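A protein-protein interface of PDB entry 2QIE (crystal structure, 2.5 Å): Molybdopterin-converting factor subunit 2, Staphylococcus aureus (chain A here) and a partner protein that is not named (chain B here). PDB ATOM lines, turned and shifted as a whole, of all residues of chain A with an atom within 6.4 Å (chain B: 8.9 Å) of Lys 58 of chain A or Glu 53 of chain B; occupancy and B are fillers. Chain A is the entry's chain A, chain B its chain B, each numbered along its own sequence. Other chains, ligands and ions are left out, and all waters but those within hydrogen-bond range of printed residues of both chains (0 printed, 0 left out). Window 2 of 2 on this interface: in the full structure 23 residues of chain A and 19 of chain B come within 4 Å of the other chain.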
ATOM      1  N   TYR A  52       3.278  10.106 -17.920  1.00  0.00           N
ATOM      2  CA  TYR A  52       2.130   9.462 -18.539  1.00  0.00           C
ATOM      3  C   TYR A  52       2.695   8.682 -19.723  1.00  0.00           C
ATOM      4  O   TYR A  52       2.790   9.197 -20.842  1.00  0.00           O
ATOM      5  CB  TYR A  52       1.101  10.512 -18.952  1.00  0.00           C
ATOM      6  CG  TYR A  52      -0.210   9.997 -19.520  1.00  0.00           C
ATOM      7  CD1 TYR A  52      -0.615   8.674 -19.357  1.00  0.00           C
ATOM      8  CD2 TYR A  52      -1.063  10.863 -20.198  1.00  0.00           C
ATOM      9  CE1 TYR A  52      -1.820   8.230 -19.873  1.00  0.00           C
ATOM     10  CE2 TYR A  52      -2.255  10.434 -20.718  1.00  0.00           C
ATOM     11  CZ  TYR A  52      -2.638   9.118 -20.553  1.00  0.00           C
ATOM     12  OH  TYR A  52      -3.839   8.690 -21.061  1.00  0.00           O
ATOM     13  N   ILE A  53       3.082   7.439 -19.444  1.00  0.00           N
ATOM     14  CA  ILE A  53       3.960   6.649 -20.335  1.00  0.00           C
ATOM     15  C   ILE A  53       3.476   6.556 -21.783  1.00  0.00           C
ATOM     16  O   ILE A  53       4.206   6.933 -22.685  1.00  0.00           O
ATOM     17  CB  ILE A  53       4.236   5.209 -19.782  1.00  0.00           C
ATOM     18  CG1 ILE A  53       5.000   5.279 -18.454  1.00  0.00           C
ATOM     19  CG2 ILE A  53       5.032   4.387 -20.803  1.00  0.00           C
ATOM     20  CD1 ILE A  53       5.023   3.987 -17.691  1.00  0.00           C
ATOM     21  N   PRO A  54       2.255   6.049 -22.009  1.00  0.00           N
ATOM     22  CA  PRO A  54       1.803   5.900 -23.391  1.00  0.00           C
ATOM     23  C   PRO A  54       1.694   7.214 -24.164  1.00  0.00           C
ATOM     24  O   PRO A  54       1.945   7.237 -25.363  1.00  0.00           O
ATOM     25  CB  PRO A  54       0.427   5.225 -23.240  1.00  0.00           C
ATOM     26  CG  PRO A  54       0.011   5.485 -21.868  1.00  0.00           C
ATOM     27  CD  PRO A  54       1.245   5.564 -21.051  1.00  0.00           C
ATOM     28  N   MET A  55       1.334   8.294 -23.489  1.00  0.00           N
ATOM     29  CA  MET A  55       1.271   9.601 -24.134  1.00  0.00           C
ATOM     30  C   MET A  55       2.667  10.177 -24.328  1.00  0.00           C
ATOM     31  O   MET A  55       2.955  10.796 -25.359  1.00  0.00           O
ATOM     32  CB  MET A  55       0.419  10.587 -23.327  1.00  0.00           C
ATOM     33  CG  MET A  55       0.206  11.906 -24.054  1.00  0.00           C
ATOM     34  SD  MET A  55      -1.102  12.948 -23.387  1.00  0.00           S
ATOM     35  CE  MET A  55      -1.011  14.337 -24.509  1.00  0.00           C
ATOM     36  N   ALA A  56       3.528   9.993 -23.333  1.00  0.00           N
ATOM     37  CA  ALA A  56       4.887  10.515 -23.419  1.00  0.00           C
ATOM     38  C   ALA A  56       5.612   9.831 -24.574  1.00  0.00           C
ATOM     39  O   ALA A  56       6.331  10.472 -25.314  1.00  0.00           O
ATOM     40  CB  ALA A  56       5.636  10.339 -22.098  1.00  0.00           C
ATOM     41  N   GLU A  57       5.392   8.535 -24.755  1.00  0.00           N
ATOM     42  CA  GLU A  57       6.010   7.820 -25.874  1.00  0.00           C
ATOM     43  C   GLU A  57       5.435   8.279 -27.226  1.00  0.00           C
ATOM     44  O   GLU A  57       6.180   8.440 -28.191  1.00  0.00           O
ATOM     45  CB  GLU A  57       5.914   6.293 -25.675  1.00  0.00           C
ATOM     46  CG  GLU A  57       6.770   5.782 -24.481  1.00  0.00           C
ATOM     47  CD  GLU A  57       6.880   4.253 -24.364  1.00  0.00           C
ATOM     48  OE1 GLU A  57       6.027   3.524 -24.922  1.00  0.00           O
ATOM     49  OE2 GLU A  57       7.830   3.779 -23.696  1.00  0.00           O
ATOM     50  N   LYS A  58       4.123   8.515 -27.290  1.00  0.00           N
ATOM     51  CA  LYS A  58       3.523   9.145 -28.485  1.00  0.00           C
ATOM     52  C   LYS A  58       4.147  10.513 -28.810  1.00  0.00           C
ATOM     53  O   LYS A  58       4.468  10.796 -29.972  1.00  0.00           O
ATOM     54  CB  LYS A  58       2.008   9.301 -28.341  1.00  0.00           C
ATOM     55  CG  LYS A  58       1.217   8.032 -28.667  1.00  0.00           C
ATOM     56  CD  LYS A  58      -0.271   8.311 -28.763  1.00  0.00           C
ATOM     57  CE  LYS A  58      -1.067   7.056 -29.133  1.00  0.00           C
ATOM     58  NZ  LYS A  58      -2.554   7.246 -28.995  1.00  0.00           N
ATOM     59  N   LYS A  59       4.319  11.345 -27.780  1.00  0.00           N
ATOM     60  CA  LYS A  59       4.834  12.709 -27.953  1.00  0.00           C
ATOM     61  C   LYS A  59       6.304  12.731 -28.377  1.00  0.00           C
ATOM     62  O   LYS A  59       6.742  13.624 -29.115  1.00  0.00           O
ATOM     63  CB  LYS A  59       4.650  13.515 -26.660  1.00  0.00           C
ATOM     64  CG  LYS A  59       3.209  13.885 -26.375  1.00  0.00           C
ATOM     65  CD  LYS A  59       2.787  15.123 -27.155  1.00  0.00           C
ATOM     66  CE  LYS A  59       1.293  15.180 -27.387  1.00  0.00           C
ATOM     67  NZ  LYS A  59       1.016  15.997 -28.581  1.00  0.00           N
ATOM     68  N   LEU A  60       7.071  11.754 -27.908  1.00  0.00           N
ATOM     69  CA  LEU A  60       8.475  11.643 -28.317  1.00  0.00           C
ATOM     70  C   LEU A  60       8.584  11.287 -29.797  1.00  0.00           C
ATOM     71  O   LEU A  60       9.400  11.844 -30.519  1.00  0.00           O
ATOM     72  CB  LEU A  60       9.198  10.627 -27.448  1.00  0.00           C
ATOM     73  CG  LEU A  60       9.396  11.057 -25.994  1.00  0.00           C
ATOM     74  CD1 LEU A  60       9.701   9.849 -25.107  1.00  0.00           C
ATOM     75  CD2 LEU A  60      10.499  12.082 -25.905  1.00  0.00           C
ATOM     76  N   ALA A  61       7.727  10.376 -30.243  1.00  0.00           N
ATOM     77  CA  ALA A  61       7.670   9.998 -31.657  1.00  0.00           C
ATOM     78  C   ALA A  61       7.231  11.171 -32.531  1.00  0.00           C
ATOM     79  O   ALA A  61       7.703  11.312 -33.660  1.00  0.00           O
ATOM     80  CB  ALA A  61       6.760   8.822 -31.861  1.00  0.00           C
ATOM     81  N   GLN A  62       6.352  12.012 -31.994  1.00  0.00           N
ATOM     82  CA  GLN A  62       5.897  13.214 -32.689  1.00  0.00           C
ATOM     83  C   GLN A  62       7.043  14.195 -32.920  1.00  0.00           C
ATOM     84  O   GLN A  62       7.054  14.933 -33.904  1.00  0.00           O
ATOM     85  CB  GLN A  62       4.799  13.902 -31.902  1.00  0.00           C
ATOM     86  CG  GLN A  62       4.158  15.085 -32.605  1.00  0.00           C
ATOM     87  CD  GLN A  62       3.212  15.837 -31.694  1.00  0.00           C
ATOM     88  OE1 GLN A  62       2.361  15.243 -31.028  1.00  0.00           O
ATOM     89  NE2 GLN A  62       3.366  17.148 -31.644  1.00  0.00           N
ATOM     90  N   ILE A  63       8.011  14.197 -32.016  1.00  0.00           N
ATOM     91  CA  ILE A  63       9.181  15.050 -32.170  1.00  0.00           C
ATOM     92  C   ILE A  63      10.103  14.491 -33.248  1.00  0.00           C
ATOM     93  O   ILE A  63      10.634  15.244 -34.066  1.00  0.00           O
ATOM     94  CB  ILE A  63       9.926  15.207 -30.847  1.00  0.00           C
ATOM     95  CG1 ILE A  63       9.009  15.912 -29.834  1.00  0.00           C
ATOM     96  CG2 ILE A  63      11.251  16.003 -31.058  1.00  0.00           C
ATOM     97  CD1 ILE A  63       9.521  15.890 -28.398  1.00  0.00           C
ATOM     98  N   ASP A  65       9.088  12.914 -35.832  1.00  0.00           N
ATOM     99  CA  ASP A  65       8.411  13.365 -37.061  1.00  0.00           C
ATOM    100  C   ASP A  65       8.697  14.828 -37.414  1.00  0.00           C
ATOM    101  O   ASP A  65       8.922  15.162 -38.578  1.00  0.00           O
ATOM    102  CB  ASP A  65       6.892  13.186 -36.930  1.00  0.00           C
ATOM    103  CG  ASP A  65       6.497  11.762 -36.624  1.00  0.00           C
ATOM    104  OD1 ASP A  65       7.294  10.845 -36.952  1.00  0.00           O
ATOM    105  OD2 ASP A  65       5.404  11.558 -36.047  1.00  0.00           O
ATOM    106  N   LEU B   4      -7.120  10.321 -14.812  1.00  0.00           N
ATOM    107  CA  LEU B   4      -5.748  10.075 -14.322  1.00  0.00           C
ATOM    108  C   LEU B   4      -5.129  11.360 -13.765  1.00  0.00           C
ATOM    109  O   LEU B   4      -5.288  12.437 -14.349  1.00  0.00           O
ATOM    110  CB  LEU B   4      -4.851   9.535 -15.435  1.00  0.00           C
ATOM    111  CG  LEU B   4      -5.280   8.256 -16.147  1.00  0.00           C
ATOM    112  CD1 LEU B   4      -4.273   7.898 -17.236  1.00  0.00           C
ATOM    113  CD2 LEU B   4      -5.431   7.098 -15.170  1.00  0.00           C
ATOM    114  N   VAL B  49      -5.786  19.404 -20.218  1.00  0.00           N
ATOM    115  CA  VAL B  49      -6.504  18.130 -20.179  1.00  0.00           C
ATOM    116  C   VAL B  49      -6.137  17.353 -21.434  1.00  0.00           C
ATOM    117  O   VAL B  49      -6.029  17.929 -22.534  1.00  0.00           O
ATOM    118  CB  VAL B  49      -8.050  18.329 -20.133  1.00  0.00           C
ATOM    119  CG1 VAL B  49      -8.776  17.010 -20.230  1.00  0.00           C
ATOM    120  CG2 VAL B  49      -8.469  19.060 -18.866  1.00  0.00           C
ATOM    121  N   ALA B  50      -5.920  16.052 -21.264  1.00  0.00           N
ATOM    122  CA  ALA B  50      -5.672  15.155 -22.392  1.00  0.00           C
ATOM    123  C   ALA B  50      -6.811  14.154 -22.472  1.00  0.00           C
ATOM    124  O   ALA B  50      -7.165  13.537 -21.471  1.00  0.00           O
ATOM    125  CB  ALA B  50      -4.350  14.441 -22.224  1.00  0.00           C
ATOM    126  N   VAL B  51      -7.407  14.015 -23.649  1.00  0.00           N
ATOM    127  CA  VAL B  51      -8.457  13.008 -23.858  1.00  0.00           C
ATOM    128  C   VAL B  51      -7.896  11.928 -24.772  1.00  0.00           C
ATOM    129  O   VAL B  51      -7.542  12.196 -25.912  1.00  0.00           O
ATOM    130  CB  VAL B  51      -9.740  13.618 -24.455  1.00  0.00           C
ATOM    131  CG1 VAL B  51     -10.753  12.539 -24.799  1.00  0.00           C
ATOM    132  CG2 VAL B  51     -10.339  14.563 -23.480  1.00  0.00           C
ATOM    133  N   ASN B  52      -7.806  10.716 -24.247  1.00  0.00           N
ATOM    134  CA  ASN B  52      -7.230   9.594 -24.967  1.00  0.00           C
ATOM    135  C   ASN B  52      -5.870   9.957 -25.565  1.00  0.00           C
ATOM    136  O   ASN B  52      -5.630   9.769 -26.757  1.00  0.00           O
ATOM    137  CB  ASN B  52      -8.198   9.089 -26.038  1.00  0.00           C
ATOM    138  CG  ASN B  52      -9.548   8.650 -25.453  1.00  0.00           C
ATOM    139  OD1 ASN B  52      -9.615   8.041 -24.380  1.00  0.00           O
ATOM    140  ND2 ASN B  52     -10.623   8.965 -26.162  1.00  0.00           N
ATOM    141  N   GLU B  53      -5.009  10.519 -24.717  1.00  0.00           N
ATOM    142  CA  GLU B  53      -3.590  10.728 -25.021  1.00  0.00           C
ATOM    143  C   GLU B  53      -3.327  11.815 -26.080  1.00  0.00           C
ATOM    144  O   GLU B  53      -2.268  11.849 -26.699  1.00  0.00           O
ATOM    145  CB  GLU B  53      -2.927   9.386 -25.401  1.00  0.00           C
ATOM    146  CG  GLU B  53      -3.144   8.272 -24.361  1.00  0.00           C
ATOM    147  CD  GLU B  53      -2.617   6.900 -24.791  1.00  0.00           C
ATOM    148  OE1 GLU B  53      -1.888   6.799 -25.804  1.00  0.00           O
ATOM    149  OE2 GLU B  53      -2.934   5.910 -24.098  1.00  0.00           O
ATOM    150  N   GLU B  54      -4.299  12.701 -26.276  1.00  0.00           N
ATOM    151  CA  GLU B  54      -4.098  13.928 -27.048  1.00  0.00           C
ATOM    152  C   GLU B  54      -4.635  15.128 -26.283  1.00  0.00           C
ATOM    153  O   GLU B  54      -5.665  15.042 -25.597  1.00  0.00           O
ATOM    154  CB  GLU B  54      -4.760  13.849 -28.429  1.00  0.00           C
ATOM    155  CG  GLU B  54      -3.785  13.549 -29.564  1.00  0.00           C
ATOM    156  CD  GLU B  54      -2.790  14.693 -29.849  1.00  0.00           C
ATOM    157  OE1 GLU B  54      -2.423  15.478 -28.917  1.00  0.00           O
ATOM    158  OE2 GLU B  54      -2.367  14.796 -31.032  1.00  0.00           O
ATOM    159  N   PHE B  55      -3.921  16.243 -26.385  1.00  0.00           N
ATOM    160  CA  PHE B  55      -4.358  17.494 -25.762  1.00  0.00           C
ATOM    161  C   PHE B  55      -5.602  18.016 -26.476  1.00  0.00           C
ATOM    162  O   PHE B  55      -5.707  17.918 -27.709  1.00  0.00           O
ATOM    163  CB  PHE B  55      -3.260  18.557 -25.849  1.00  0.00           C
ATOM    164  CG  PHE B  55      -2.064  18.276 -24.984  1.00  0.00           C
ATOM    165  CD1 PHE B  55      -0.823  18.029 -25.555  1.00  0.00           C
ATOM    166  CD2 PHE B  55      -2.178  18.270 -23.587  1.00  0.00           C
ATOM    167  CE1 PHE B  55       0.272  17.775 -24.764  1.00  0.00           C
ATOM    168  CE2 PHE B  55      -1.069  18.025 -22.784  1.00  0.00           C
ATOM    169  CZ  PHE B  55       0.149  17.770 -23.371  1.00  0.00           C
ATOM    170  N   VAL B  56      -6.515  18.602 -25.708  1.00  0.00           N
ATOM    171  CA  VAL B  56      -7.761  19.140 -26.266  1.00  0.00           C
ATOM    172  C   VAL B  56      -8.103  20.546 -25.784  1.00  0.00           C
ATOM    173  O   VAL B  56      -7.533  21.033 -24.809  1.00  0.00           O
ATOM    174  CB  VAL B  56      -8.952  18.209 -25.971  1.00  0.00           C
ATOM    175  CG1 VAL B  56      -8.874  16.969 -26.846  1.00  0.00           C
ATOM    176  CG2 VAL B  56      -8.985  17.831 -24.513  1.00  0.00           C
ATOM    177  N   ASP B  66     -14.216   7.414 -22.433  1.00  0.00           N
ATOM    178  CA  ASP B  66     -12.907   8.005 -22.711  1.00  0.00           C
ATOM    179  C   ASP B  66     -11.985   7.913 -21.505  1.00  0.00           C
ATOM    180  O   ASP B  66     -12.414   7.649 -20.386  1.00  0.00           O
ATOM    181  CB  ASP B  66     -13.024   9.467 -23.185  1.00  0.00           C
ATOM    182  CG  ASP B  66     -13.381   9.591 -24.683  1.00  0.00           C
ATOM    183  OD1 ASP B  66     -13.392   8.568 -25.408  1.00  0.00           O
ATOM    184  OD2 ASP B  66     -13.644  10.731 -25.144  1.00  0.00           O
ATOM    185  N   THR B  67     -10.700   8.094 -21.774  1.00  0.00           N
ATOM    186  CA  THR B  67      -9.683   8.236 -20.742  1.00  0.00           C
ATOM    187  C   THR B  67      -9.205   9.683 -20.745  1.00  0.00           C
ATOM    188  O   THR B  67      -8.849  10.219 -21.790  1.00  0.00           O
ATOM    189  CB  THR B  67      -8.518   7.283 -21.000  1.00  0.00           C
ATOM    190  OG1 THR B  67      -8.954   5.948 -20.720  1.00  0.00           O
ATOM    191  CG2 THR B  67      -7.295   7.619 -20.122  1.00  0.00           C
ATOM    192  N   VAL B  68      -9.221  10.301 -19.569  1.00  0.00           N
ATOM    193  CA  VAL B  68      -8.929  11.723 -19.419  1.00  0.00           C
ATOM    194  C   VAL B  68      -7.770  11.908 -18.457  1.00  0.00           C
ATOM    195  O   VAL B  68      -7.652  11.190 -17.476  1.00  0.00           O
ATOM    196  CB  VAL B  68     -10.149  12.479 -18.866  1.00  0.00           C
ATOM    197  CG1 VAL B  68      -9.918  13.995 -18.925  1.00  0.00           C
ATOM    198  CG2 VAL B  68     -11.409  12.101 -19.644  1.00  0.00           C
ATOM    199  N   ALA B  69      -6.923  12.885 -18.713  1.00  0.00           N
ATOM    200  CA  ALA B  69      -5.720  13.039 -17.911  1.00  0.00           C
ATOM    201  C   ALA B  69      -5.424  14.490 -17.628  1.00  0.00           C
ATOM    202  O   ALA B  69      -5.363  15.302 -18.551  1.00  0.00           O
ATOM    203  CB  ALA B  69      -4.558  12.406 -18.612  1.00  0.00           C
ATOM    204  N   ILE B  71      -2.902  17.137 -16.940  1.00  0.00           N
ATOM    205  CA  ILE B  71      -1.482  17.309 -17.224  1.00  0.00           C
ATOM    206  C   ILE B  71      -0.989  18.643 -16.677  1.00  0.00           C
ATOM    207  O   ILE B  71      -1.152  19.656 -17.334  1.00  0.00           O
ATOM    208  CB  ILE B  71      -1.238  17.314 -18.771  1.00  0.00           C
ATOM    209  CG1 ILE B  71      -1.803  16.042 -19.415  1.00  0.00           C
ATOM    210  CG2 ILE B  71       0.228  17.463 -19.099  1.00  0.00           C
ATOM    211  CD1 ILE B  71      -1.288  14.752 -18.824  1.00  0.00           C
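The side-chain amino group (NZ) of Lys 58 of chain A lies within salt-bridge range of the side-chain carboxylate (OE1) of Glu 53 of chain B (3.3 Å).
The side-chain amino group of Lys 59 of chain A is in salt-bridge range of the side-chain carboxylate of Glu 54 of chain B (3.5 Å).
SD of Met 55 of chain A sits close to O of Glu 53 of chain B.
Among the printed residues, pairs that only touch across the chains: Tyr 52 of chain A with Leu 4 of chain B (3.6 Å), Tyr 52 of chain A with Glu 53 of chain B (3.4 Å), Tyr 52 of chain A with Thr 67 of chain B (3.7 Å), Tyr 52 of chain A with Ala 69 of chain B (3.7 Å), Pro 54 of chain A with Glu 53 of chain B (3.5 Å), Met 55 of chain A with Ala 50 of chain B (3.8 Å), Met 55 of chain A with Phe 55 of chain B (3.7 Å) and Lys 59 of chain A with Phe 55 of chain B (3.8 Å).
Of the printed residues of chain B, Met 55 of chain A touches Ala 50 (3.8 Å), Glu 53 (3.5 Å) and Phe 55 (3.7 Å).
Lys 58 of chain A touches one residue of chain B.
Gln 62 of chain A touches none of the printed residues of chain B.
Of the printed residues of chain A, Leu 4 of chain B touches Tyr 52 (3.6 Å).
Printed residues of chain A within 4 Å of Ala 50 of chain B: Met 55 (3.8 Å).
Of chain A, only Tyr 52 (3.4 Å), Pro 54 (3.5 Å), Met 55 (3.5 Å) and Lys 58 (3.3 Å) come within 4 Å of Glu 53 of chain B.
Printed residues of chain A within 4 Å of Glu 54 of chain B: Lys 59 (3.5 Å).
Of the printed residues of chain A, Phe 55 of chain B touches Met 55 and Lys 59.
The nearest residue of chain B that does not touch Lys 58 of chain A is Asn 52 of chain B (4.6 Å).
The nearest residue of chain A that does not touch Glu 53 of chain B is Lys 59 of chain A (4.9 Å).
Of the 13 printed residues of chain A, 5 touch a printed residue of chain B.
Hydrophobic or aromatic side chains of chain A within 4 Å of the printed part of chain B: Tyr 52, Pro 54 and Met 55.
Along chain A the printed residues that touch a printed residue of chain B span positions 52 to 59.
Printed residues of chain B that touch a printed residue of chain A: Leu 4, Ala 50, Glu 53, Glu 54, Phe 55, Thr 67 and Ala 69.
Among the printed residues, 11 pairs touch across the chains.
Among the printed residues, Asp or Glu carboxylates within 4 Å of a Lys or Arg side-chain nitrogen of the other chain: Lys 58 of chain A with Glu 53 of chain B (3.3 Å) and Lys 59 of chain A with Glu 54 of chain B (3.5 Å).
The side-chain amino group (NZ) of Lys 59 of chain A lies within hydrogen-bond range of the side-chain amide oxygen (OE1) of Gln 62 of chain A (2.9 Å).
The backbone NH (N) of Leu 4 of chain B is in hydrogen-bond range of the backbone carbonyl oxygen (O) of Val 68 of chain B (2.9 Å).
The backbone carbonyl oxygen (O) of Ala 50 of chain B is in hydrogen-bond range of the backbone NH (N) of Ala 69 of chain B (2.8 Å).
O of Thr 67 of chain B lies within hydrogen-bond range of N of Asn 52 of chain B (2.7 Å).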
